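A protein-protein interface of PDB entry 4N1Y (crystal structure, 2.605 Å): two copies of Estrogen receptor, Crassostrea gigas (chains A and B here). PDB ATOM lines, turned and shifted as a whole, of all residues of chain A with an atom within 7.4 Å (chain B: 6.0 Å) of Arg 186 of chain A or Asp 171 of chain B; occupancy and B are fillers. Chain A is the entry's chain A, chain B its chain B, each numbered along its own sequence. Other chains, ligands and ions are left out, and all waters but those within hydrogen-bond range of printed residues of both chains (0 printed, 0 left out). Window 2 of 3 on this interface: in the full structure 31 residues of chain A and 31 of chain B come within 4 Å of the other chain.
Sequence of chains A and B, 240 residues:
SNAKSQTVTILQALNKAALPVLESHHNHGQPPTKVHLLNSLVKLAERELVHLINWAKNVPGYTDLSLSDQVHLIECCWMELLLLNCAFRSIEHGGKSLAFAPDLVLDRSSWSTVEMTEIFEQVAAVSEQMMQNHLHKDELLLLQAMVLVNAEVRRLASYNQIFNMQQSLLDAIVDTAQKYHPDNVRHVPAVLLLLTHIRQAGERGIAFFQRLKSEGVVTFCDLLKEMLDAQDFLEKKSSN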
ATOM      1  N   ASN A 133      -8.841  32.774 -25.223  1.00  0.00           N
ATOM      2  CA  ASN A 133      -7.823  32.461 -24.230  1.00  0.00           C
ATOM      3  C   ASN A 133      -7.784  33.503 -23.122  1.00  0.00           C
ATOM      4  O   ASN A 133      -6.881  33.488 -22.280  1.00  0.00           O
ATOM      5  CB  ASN A 133      -6.431  32.348 -24.869  1.00  0.00           C
ATOM      6  CG  ASN A 133      -6.245  31.059 -25.650  1.00  0.00           C
ATOM      7  OD1 ASN A 133      -6.190  29.979 -25.068  1.00  0.00           O
ATOM      8  ND2 ASN A 133      -6.077  31.173 -26.961  1.00  0.00           N
ATOM      9  N   ASP A 183      -1.592  27.692 -13.210  1.00  0.00           N
ATOM     10  CA  ASP A 183      -1.483  26.223 -13.289  1.00  0.00           C
ATOM     11  C   ASP A 183      -1.966  25.615 -14.604  1.00  0.00           C
ATOM     12  O   ASP A 183      -2.068  24.393 -14.747  1.00  0.00           O
ATOM     13  CB  ASP A 183      -2.230  25.593 -12.120  1.00  0.00           C
ATOM     14  CG  ASP A 183      -1.664  26.029 -10.795  1.00  0.00           C
ATOM     15  OD1 ASP A 183      -0.488  26.467 -10.784  1.00  0.00           O
ATOM     16  OD2 ASP A 183      -2.400  25.977  -9.784  1.00  0.00           O
ATOM     17  N   ASN A 184      -2.248  26.481 -15.562  1.00  0.00           N
ATOM     18  CA  ASN A 184      -2.645  26.066 -16.894  1.00  0.00           C
ATOM     19  C   ASN A 184      -1.424  25.839 -17.798  1.00  0.00           C
ATOM     20  O   ASN A 184      -0.824  26.805 -18.303  1.00  0.00           O
ATOM     21  CB  ASN A 184      -3.576  27.114 -17.479  1.00  0.00           C
ATOM     22  CG  ASN A 184      -4.251  26.655 -18.734  1.00  0.00           C
ATOM     23  OD1 ASN A 184      -3.771  25.759 -19.430  1.00  0.00           O
ATOM     24  ND2 ASN A 184      -5.385  27.268 -19.036  1.00  0.00           N
ATOM     25  N   VAL A 185      -1.062  24.569 -17.997  1.00  0.00           N
ATOM     26  CA  VAL A 185       0.142  24.244 -18.747  1.00  0.00           C
ATOM     27  C   VAL A 185      -0.009  24.488 -20.243  1.00  0.00           C
ATOM     28  O   VAL A 185       0.982  24.683 -20.948  1.00  0.00           O
ATOM     29  CB  VAL A 185       0.552  22.768 -18.562  1.00  0.00           C
ATOM     30  CG1 VAL A 185       0.712  22.438 -17.090  1.00  0.00           C
ATOM     31  CG2 VAL A 185      -0.462  21.847 -19.216  1.00  0.00           C
ATOM     32  N   ARG A 186      -1.250  24.550 -20.707  1.00  0.00           N
ATOM     33  CA  ARG A 186      -1.517  24.678 -22.125  1.00  0.00           C
ATOM     34  C   ARG A 186      -1.562  26.121 -22.566  1.00  0.00           C
ATOM     35  O   ARG A 186      -1.511  26.380 -23.755  1.00  0.00           O
ATOM     36  CB  ARG A 186      -2.839  24.016 -22.497  1.00  0.00           C
ATOM     37  CG  ARG A 186      -2.922  22.546 -22.227  1.00  0.00           C
ATOM     38  CD  ARG A 186      -4.377  22.160 -22.265  1.00  0.00           C
ATOM     39  NE  ARG A 186      -4.587  20.759 -21.959  1.00  0.00           N
ATOM     40  CZ  ARG A 186      -5.778  20.175 -21.986  1.00  0.00           C
ATOM     41  NH1 ARG A 186      -6.849  20.892 -22.300  1.00  0.00           N
ATOM     42  NH2 ARG A 186      -5.905  18.882 -21.701  1.00  0.00           N
ATOM     43  N   HIS A 187      -1.679  27.055 -21.625  1.00  0.00           N
ATOM     44  CA  HIS A 187      -1.920  28.452 -21.991  1.00  0.00           C
ATOM     45  C   HIS A 187      -0.808  29.059 -22.830  1.00  0.00           C
ATOM     46  O   HIS A 187      -1.059  29.546 -23.925  1.00  0.00           O
ATOM     47  CB  HIS A 187      -2.121  29.322 -20.762  1.00  0.00           C
ATOM     48  CG  HIS A 187      -2.418  30.749 -21.091  1.00  0.00           C
ATOM     49  ND1 HIS A 187      -3.667  31.172 -21.502  1.00  0.00           N
ATOM     50  CD2 HIS A 187      -1.630  31.849 -21.096  1.00  0.00           C
ATOM     51  CE1 HIS A 187      -3.640  32.475 -21.718  1.00  0.00           C
ATOM     52  NE2 HIS A 187      -2.415  32.909 -21.485  1.00  0.00           N
ATOM     53  N   VAL A 188       0.416  29.049 -22.314  1.00  0.00           N
ATOM     54  CA  VAL A 188       1.534  29.626 -23.051  1.00  0.00           C
ATOM     55  C   VAL A 188       1.743  28.991 -24.434  1.00  0.00           C
ATOM     56  O   VAL A 188       1.847  29.712 -25.427  1.00  0.00           O
ATOM     57  CB  VAL A 188       2.830  29.530 -22.245  1.00  0.00           C
ATOM     58  CG1 VAL A 188       4.010  29.970 -23.086  1.00  0.00           C
ATOM     59  CG2 VAL A 188       2.726  30.406 -21.044  1.00  0.00           C
ATOM     60  N   PRO A 189       1.771  27.650 -24.515  1.00  0.00           N
ATOM     61  CA  PRO A 189       1.994  27.069 -25.839  1.00  0.00           C
ATOM     62  C   PRO A 189       0.926  27.437 -26.837  1.00  0.00           C
ATOM     63  O   PRO A 189       1.267  27.905 -27.919  1.00  0.00           O
ATOM     64  CB  PRO A 189       1.945  25.575 -25.575  1.00  0.00           C
ATOM     65  CG  PRO A 189       2.272  25.436 -24.135  1.00  0.00           C
ATOM     66  CD  PRO A 189       1.653  26.608 -23.484  1.00  0.00           C
ATOM     67  N   ALA A 190      -0.338  27.271 -26.465  1.00  0.00           N
ATOM     68  CA  ALA A 190      -1.430  27.564 -27.386  1.00  0.00           C
ATOM     69  C   ALA A 190      -1.307  29.005 -27.865  1.00  0.00           C
ATOM     70  O   ALA A 190      -1.481  29.300 -29.049  1.00  0.00           O
ATOM     71  CB  ALA A 190      -2.792  27.324 -26.738  1.00  0.00           C
ATOM     72  N   VAL A 191      -1.004  29.902 -26.944  1.00  0.00           N
ATOM     73  CA  VAL A 191      -0.905  31.298 -27.296  1.00  0.00           C
ATOM     74  C   VAL A 191       0.259  31.578 -28.253  1.00  0.00           C
ATOM     75  O   VAL A 191       0.103  32.305 -29.235  1.00  0.00           O
ATOM     76  CB  VAL A 191      -0.743  32.154 -26.043  1.00  0.00           C
ATOM     77  CG1 VAL A 191      -0.248  33.557 -26.393  1.00  0.00           C
ATOM     78  CG2 VAL A 191      -2.051  32.186 -25.262  1.00  0.00           C
ATOM     79  N   LEU A 192       1.421  31.000 -27.978  1.00  0.00           N
ATOM     80  CA  LEU A 192       2.559  31.170 -28.861  1.00  0.00           C
ATOM     81  C   LEU A 192       2.266  30.643 -30.257  1.00  0.00           C
ATOM     82  O   LEU A 192       2.762  31.203 -31.222  1.00  0.00           O
ATOM     83  CB  LEU A 192       3.795  30.496 -28.281  1.00  0.00           C
ATOM     84  CG  LEU A 192       4.271  31.275 -27.063  1.00  0.00           C
ATOM     85  CD1 LEU A 192       5.590  30.756 -26.588  1.00  0.00           C
ATOM     86  CD2 LEU A 192       4.346  32.760 -27.377  1.00  0.00           C
ATOM     87  N   THR B   7      -0.566  11.281 -23.368  1.00  0.00           N
ATOM     88  CA  THR B   7       0.753  11.614 -23.866  1.00  0.00           C
ATOM     89  C   THR B   7       1.446  10.337 -24.343  1.00  0.00           C
ATOM     90  O   THR B   7       2.060  10.289 -25.419  1.00  0.00           O
ATOM     91  CB  THR B   7       1.588  12.274 -22.764  1.00  0.00           C
ATOM     92  OG1 THR B   7       1.646  11.382 -21.646  1.00  0.00           O
ATOM     93  CG2 THR B   7       0.927  13.559 -22.295  1.00  0.00           C
ATOM     94  N   GLN B 166      -5.610  19.414 -30.655  1.00  0.00           N
ATOM     95  CA  GLN B 166      -4.673  20.444 -30.223  1.00  0.00           C
ATOM     96  C   GLN B 166      -4.416  20.388 -28.707  1.00  0.00           C
ATOM     97  O   GLN B 166      -3.272  20.449 -28.259  1.00  0.00           O
ATOM     98  CB  GLN B 166      -5.193  21.830 -30.618  1.00  0.00           C
ATOM     99  CG  GLN B 166      -4.251  22.980 -30.240  1.00  0.00           C
ATOM    100  CD  GLN B 166      -4.930  24.339 -30.272  1.00  0.00           C
ATOM    101  OE1 GLN B 166      -6.078  24.464 -30.712  1.00  0.00           O
ATOM    102  NE2 GLN B 166      -4.240  25.355 -29.767  1.00  0.00           N
ATOM    103  N   GLN B 167      -5.482  20.253 -27.928  1.00  0.00           N
ATOM    104  CA  GLN B 167      -5.359  20.154 -26.487  1.00  0.00           C
ATOM    105  C   GLN B 167      -4.551  18.929 -26.111  1.00  0.00           C
ATOM    106  O   GLN B 167      -3.661  19.009 -25.259  1.00  0.00           O
ATOM    107  CB  GLN B 167      -6.737  20.137 -25.831  1.00  0.00           C
ATOM    108  CG  GLN B 167      -7.490  21.441 -26.041  1.00  0.00           C
ATOM    109  CD  GLN B 167      -6.670  22.650 -25.631  1.00  0.00           C
ATOM    110  OE1 GLN B 167      -6.492  22.918 -24.449  1.00  0.00           O
ATOM    111  NE2 GLN B 167      -6.142  23.368 -26.611  1.00  0.00           N
ATOM    112  N   SER B 168      -4.841  17.797 -26.747  1.00  0.00           N
ATOM    113  CA  SER B 168      -4.093  16.586 -26.428  1.00  0.00           C
ATOM    114  C   SER B 168      -2.638  16.746 -26.834  1.00  0.00           C
ATOM    115  O   SER B 168      -1.743  16.371 -26.080  1.00  0.00           O
ATOM    116  CB  SER B 168      -4.669  15.352 -27.124  1.00  0.00           C
ATOM    117  OG  SER B 168      -6.001  15.091 -26.726  1.00  0.00           O
ATOM    118  N   LEU B 169      -2.392  17.337 -28.003  1.00  0.00           N
ATOM    119  CA  LEU B 169      -1.015  17.528 -28.443  1.00  0.00           C
ATOM    120  C   LEU B 169      -0.255  18.475 -27.514  1.00  0.00           C
ATOM    121  O   LEU B 169       0.876  18.184 -27.124  1.00  0.00           O
ATOM    122  CB  LEU B 169      -0.983  18.031 -29.880  1.00  0.00           C
ATOM    123  CG  LEU B 169      -1.338  16.885 -30.819  1.00  0.00           C
ATOM    124  CD1 LEU B 169      -1.369  17.323 -32.278  1.00  0.00           C
ATOM    125  CD2 LEU B 169      -0.375  15.742 -30.594  1.00  0.00           C
ATOM    126  N   LEU B 170      -0.896  19.567 -27.113  1.00  0.00           N
ATOM    127  CA  LEU B 170      -0.288  20.524 -26.192  1.00  0.00           C
ATOM    128  C   LEU B 170       0.144  19.864 -24.877  1.00  0.00           C
ATOM    129  O   LEU B 170       1.244  20.118 -24.386  1.00  0.00           O
ATOM    130  CB  LEU B 170      -1.257  21.653 -25.897  1.00  0.00           C
ATOM    131  CG  LEU B 170      -1.422  22.699 -26.985  1.00  0.00           C
ATOM    132  CD1 LEU B 170      -2.400  23.769 -26.524  1.00  0.00           C
ATOM    133  CD2 LEU B 170      -0.076  23.309 -27.346  1.00  0.00           C
ATOM    134  N   ASP B 171      -0.713  19.010 -24.320  1.00  0.00           N
ATOM    135  CA  ASP B 171      -0.357  18.269 -23.120  1.00  0.00           C
ATOM    136  C   ASP B 171       0.846  17.360 -23.369  1.00  0.00           C
ATOM    137  O   ASP B 171       1.756  17.299 -22.551  1.00  0.00           O
ATOM    138  CB  ASP B 171      -1.528  17.424 -22.631  1.00  0.00           C
ATOM    139  CG  ASP B 171      -2.671  18.266 -22.103  1.00  0.00           C
ATOM    140  OD1 ASP B 171      -2.457  19.482 -21.871  1.00  0.00           O
ATOM    141  OD2 ASP B 171      -3.783  17.704 -21.928  1.00  0.00           O
ATOM    142  N   ALA B 172       0.846  16.658 -24.500  1.00  0.00           N
ATOM    143  CA  ALA B 172       1.914  15.717 -24.815  1.00  0.00           C
ATOM    144  C   ALA B 172       3.263  16.425 -24.997  1.00  0.00           C
ATOM    145  O   ALA B 172       4.306  15.944 -24.552  1.00  0.00           O
ATOM    146  CB  ALA B 172       1.553  14.916 -26.044  1.00  0.00           C
ATOM    147  N   ILE B 173       3.235  17.577 -25.640  1.00  0.00           N
ATOM    148  CA  ILE B 173       4.451  18.349 -25.812  1.00  0.00           C
ATOM    149  C   ILE B 173       5.030  18.770 -24.466  1.00  0.00           C
ATOM    150  O   ILE B 173       6.229  18.631 -24.208  1.00  0.00           O
ATOM    151  CB  ILE B 173       4.178  19.581 -26.664  1.00  0.00           C
ATOM    152  CG1 ILE B 173       4.062  19.170 -28.133  1.00  0.00           C
ATOM    153  CG2 ILE B 173       5.263  20.584 -26.485  1.00  0.00           C
ATOM    154  CD1 ILE B 173       3.506  20.253 -29.031  1.00  0.00           C
ATOM    155  N   VAL B 174       4.154  19.244 -23.594  1.00  0.00           N
ATOM    156  CA  VAL B 174       4.566  19.712 -22.287  1.00  0.00           C
ATOM    157  C   VAL B 174       5.155  18.600 -21.416  1.00  0.00           C
ATOM    158  O   VAL B 174       6.191  18.780 -20.768  1.00  0.00           O
ATOM    159  CB  VAL B 174       3.381  20.353 -21.565  1.00  0.00           C
ATOM    160  CG1 VAL B 174       3.697  20.556 -20.107  1.00  0.00           C
ATOM    161  CG2 VAL B 174       3.040  21.676 -22.222  1.00  0.00           C
ATOM    162  N   ASP B 175       4.496  17.448 -21.413  1.00  0.00           N
ATOM    163  CA  ASP B 175       4.971  16.285 -20.661  1.00  0.00           C
ATOM    164  C   ASP B 175       6.262  15.745 -21.237  1.00  0.00           C
ATOM    165  O   ASP B 175       7.150  15.340 -20.498  1.00  0.00           O
ATOM    166  CB  ASP B 175       3.906  15.188 -20.626  1.00  0.00           C
ATOM    167  CG  ASP B 175       2.741  15.539 -19.713  1.00  0.00           C
ATOM    168  OD1 ASP B 175       2.732  16.670 -19.178  1.00  0.00           O
ATOM    169  OD2 ASP B 175       1.831  14.697 -19.536  1.00  0.00           O
ATOM    170  N   THR B 176       6.363  15.734 -22.563  1.00  0.00           N
ATOM    171  CA  THR B 176       7.551  15.199 -23.212  1.00  0.00           C
ATOM    172  C   THR B 176       8.736  16.110 -22.957  1.00  0.00           C
ATOM    173  O   THR B 176       9.868  15.650 -22.802  1.00  0.00           O
ATOM    174  CB  THR B 176       7.321  15.017 -24.711  1.00  0.00           C
ATOM    175  OG1 THR B 176       6.236  14.103 -24.876  1.00  0.00           O
ATOM    176  CG2 THR B 176       8.540  14.410 -25.386  1.00  0.00           C
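No position is printed for both chains.
Of the 7 pairs that touch across the chains among the printed residues, none has its exchanged pair printed and touching as well.
Among the printed residues, pairs that only touch across the chains: Pro 189 of chain A with Leu 170 of chain B (3.5 Å), Ala 190 of chain A with Leu 170 of chain B (3.6 Å), Val 185 of chain A with Val 174 of chain B (3.9 Å), Ala 190 of chain A with Gln 166 of chain B (3.9 Å) and Arg 186 of chain A with Leu 170 of chain B (3.9 Å).
Printed residues of chain B that touch a printed residue of chain A: Gln 166, Gln 167, Leu 170, Asp 171 and Val 174.
Hydrophobic or aromatic side chains of chain B within 4 Å of the printed part of chain A: Leu 170 and Val 174.
Of the 11 printed residues of chain A, 4 touch a printed residue of chain B.
Printed residues of chain A that touch a printed residue of chain B: Val 185, Arg 186, Pro 189 and Ala 190.
Hydrophobic or aromatic side chains of chain A that line the printed part of chain B: Pro 189 and Ala 190.
Among the printed residues, 7 pairs touch across the chains.
Among the printed residues, Asp or Glu carboxylates within 4 Å of a Lys or Arg side-chain nitrogen of the other chain: Arg 186 of chain A with Asp 171 of chain B (2.4 Å).
Arg 186 of chain A touches three residues of chain B.
Printed residues of chain A within 4 Å of Gln 167 of chain B: Arg 186 (3.0 Å).
Ser 168 of chain B touches none of the printed residues of chain A.
Of chain A, only Arg 186 (2.4 Å) comes within 4 Å of Asp 171 of chain B.
Printed residues of chain A within 4 Å of Val 174 of chain B: Val 185 (3.9 Å).
The nearest residue of chain B that does not touch Arg 186 of chain A is Ser 168 of chain B (5.3 Å).
The nearest printed residue of chain B that does not touch Pro 189 of chain A is Val 174 of chain B (4.3 Å).
NH1 of Arg 186 of chain A lies within hydrogen-bond range of OE1 of Gln 167 of chain B, 3.0 Å away.
The guanidinium group (NH2) of Arg 186 of chain A is in salt-bridge range of the side-chain carboxylate (OD2) of Asp 171 of chain B, 2.4 Å away.
The side-chain amide oxygen (OD1) of Asn 184 of chain A lies within hydrogen-bond range of the backbone NH (N) of Arg 186 of chain A.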
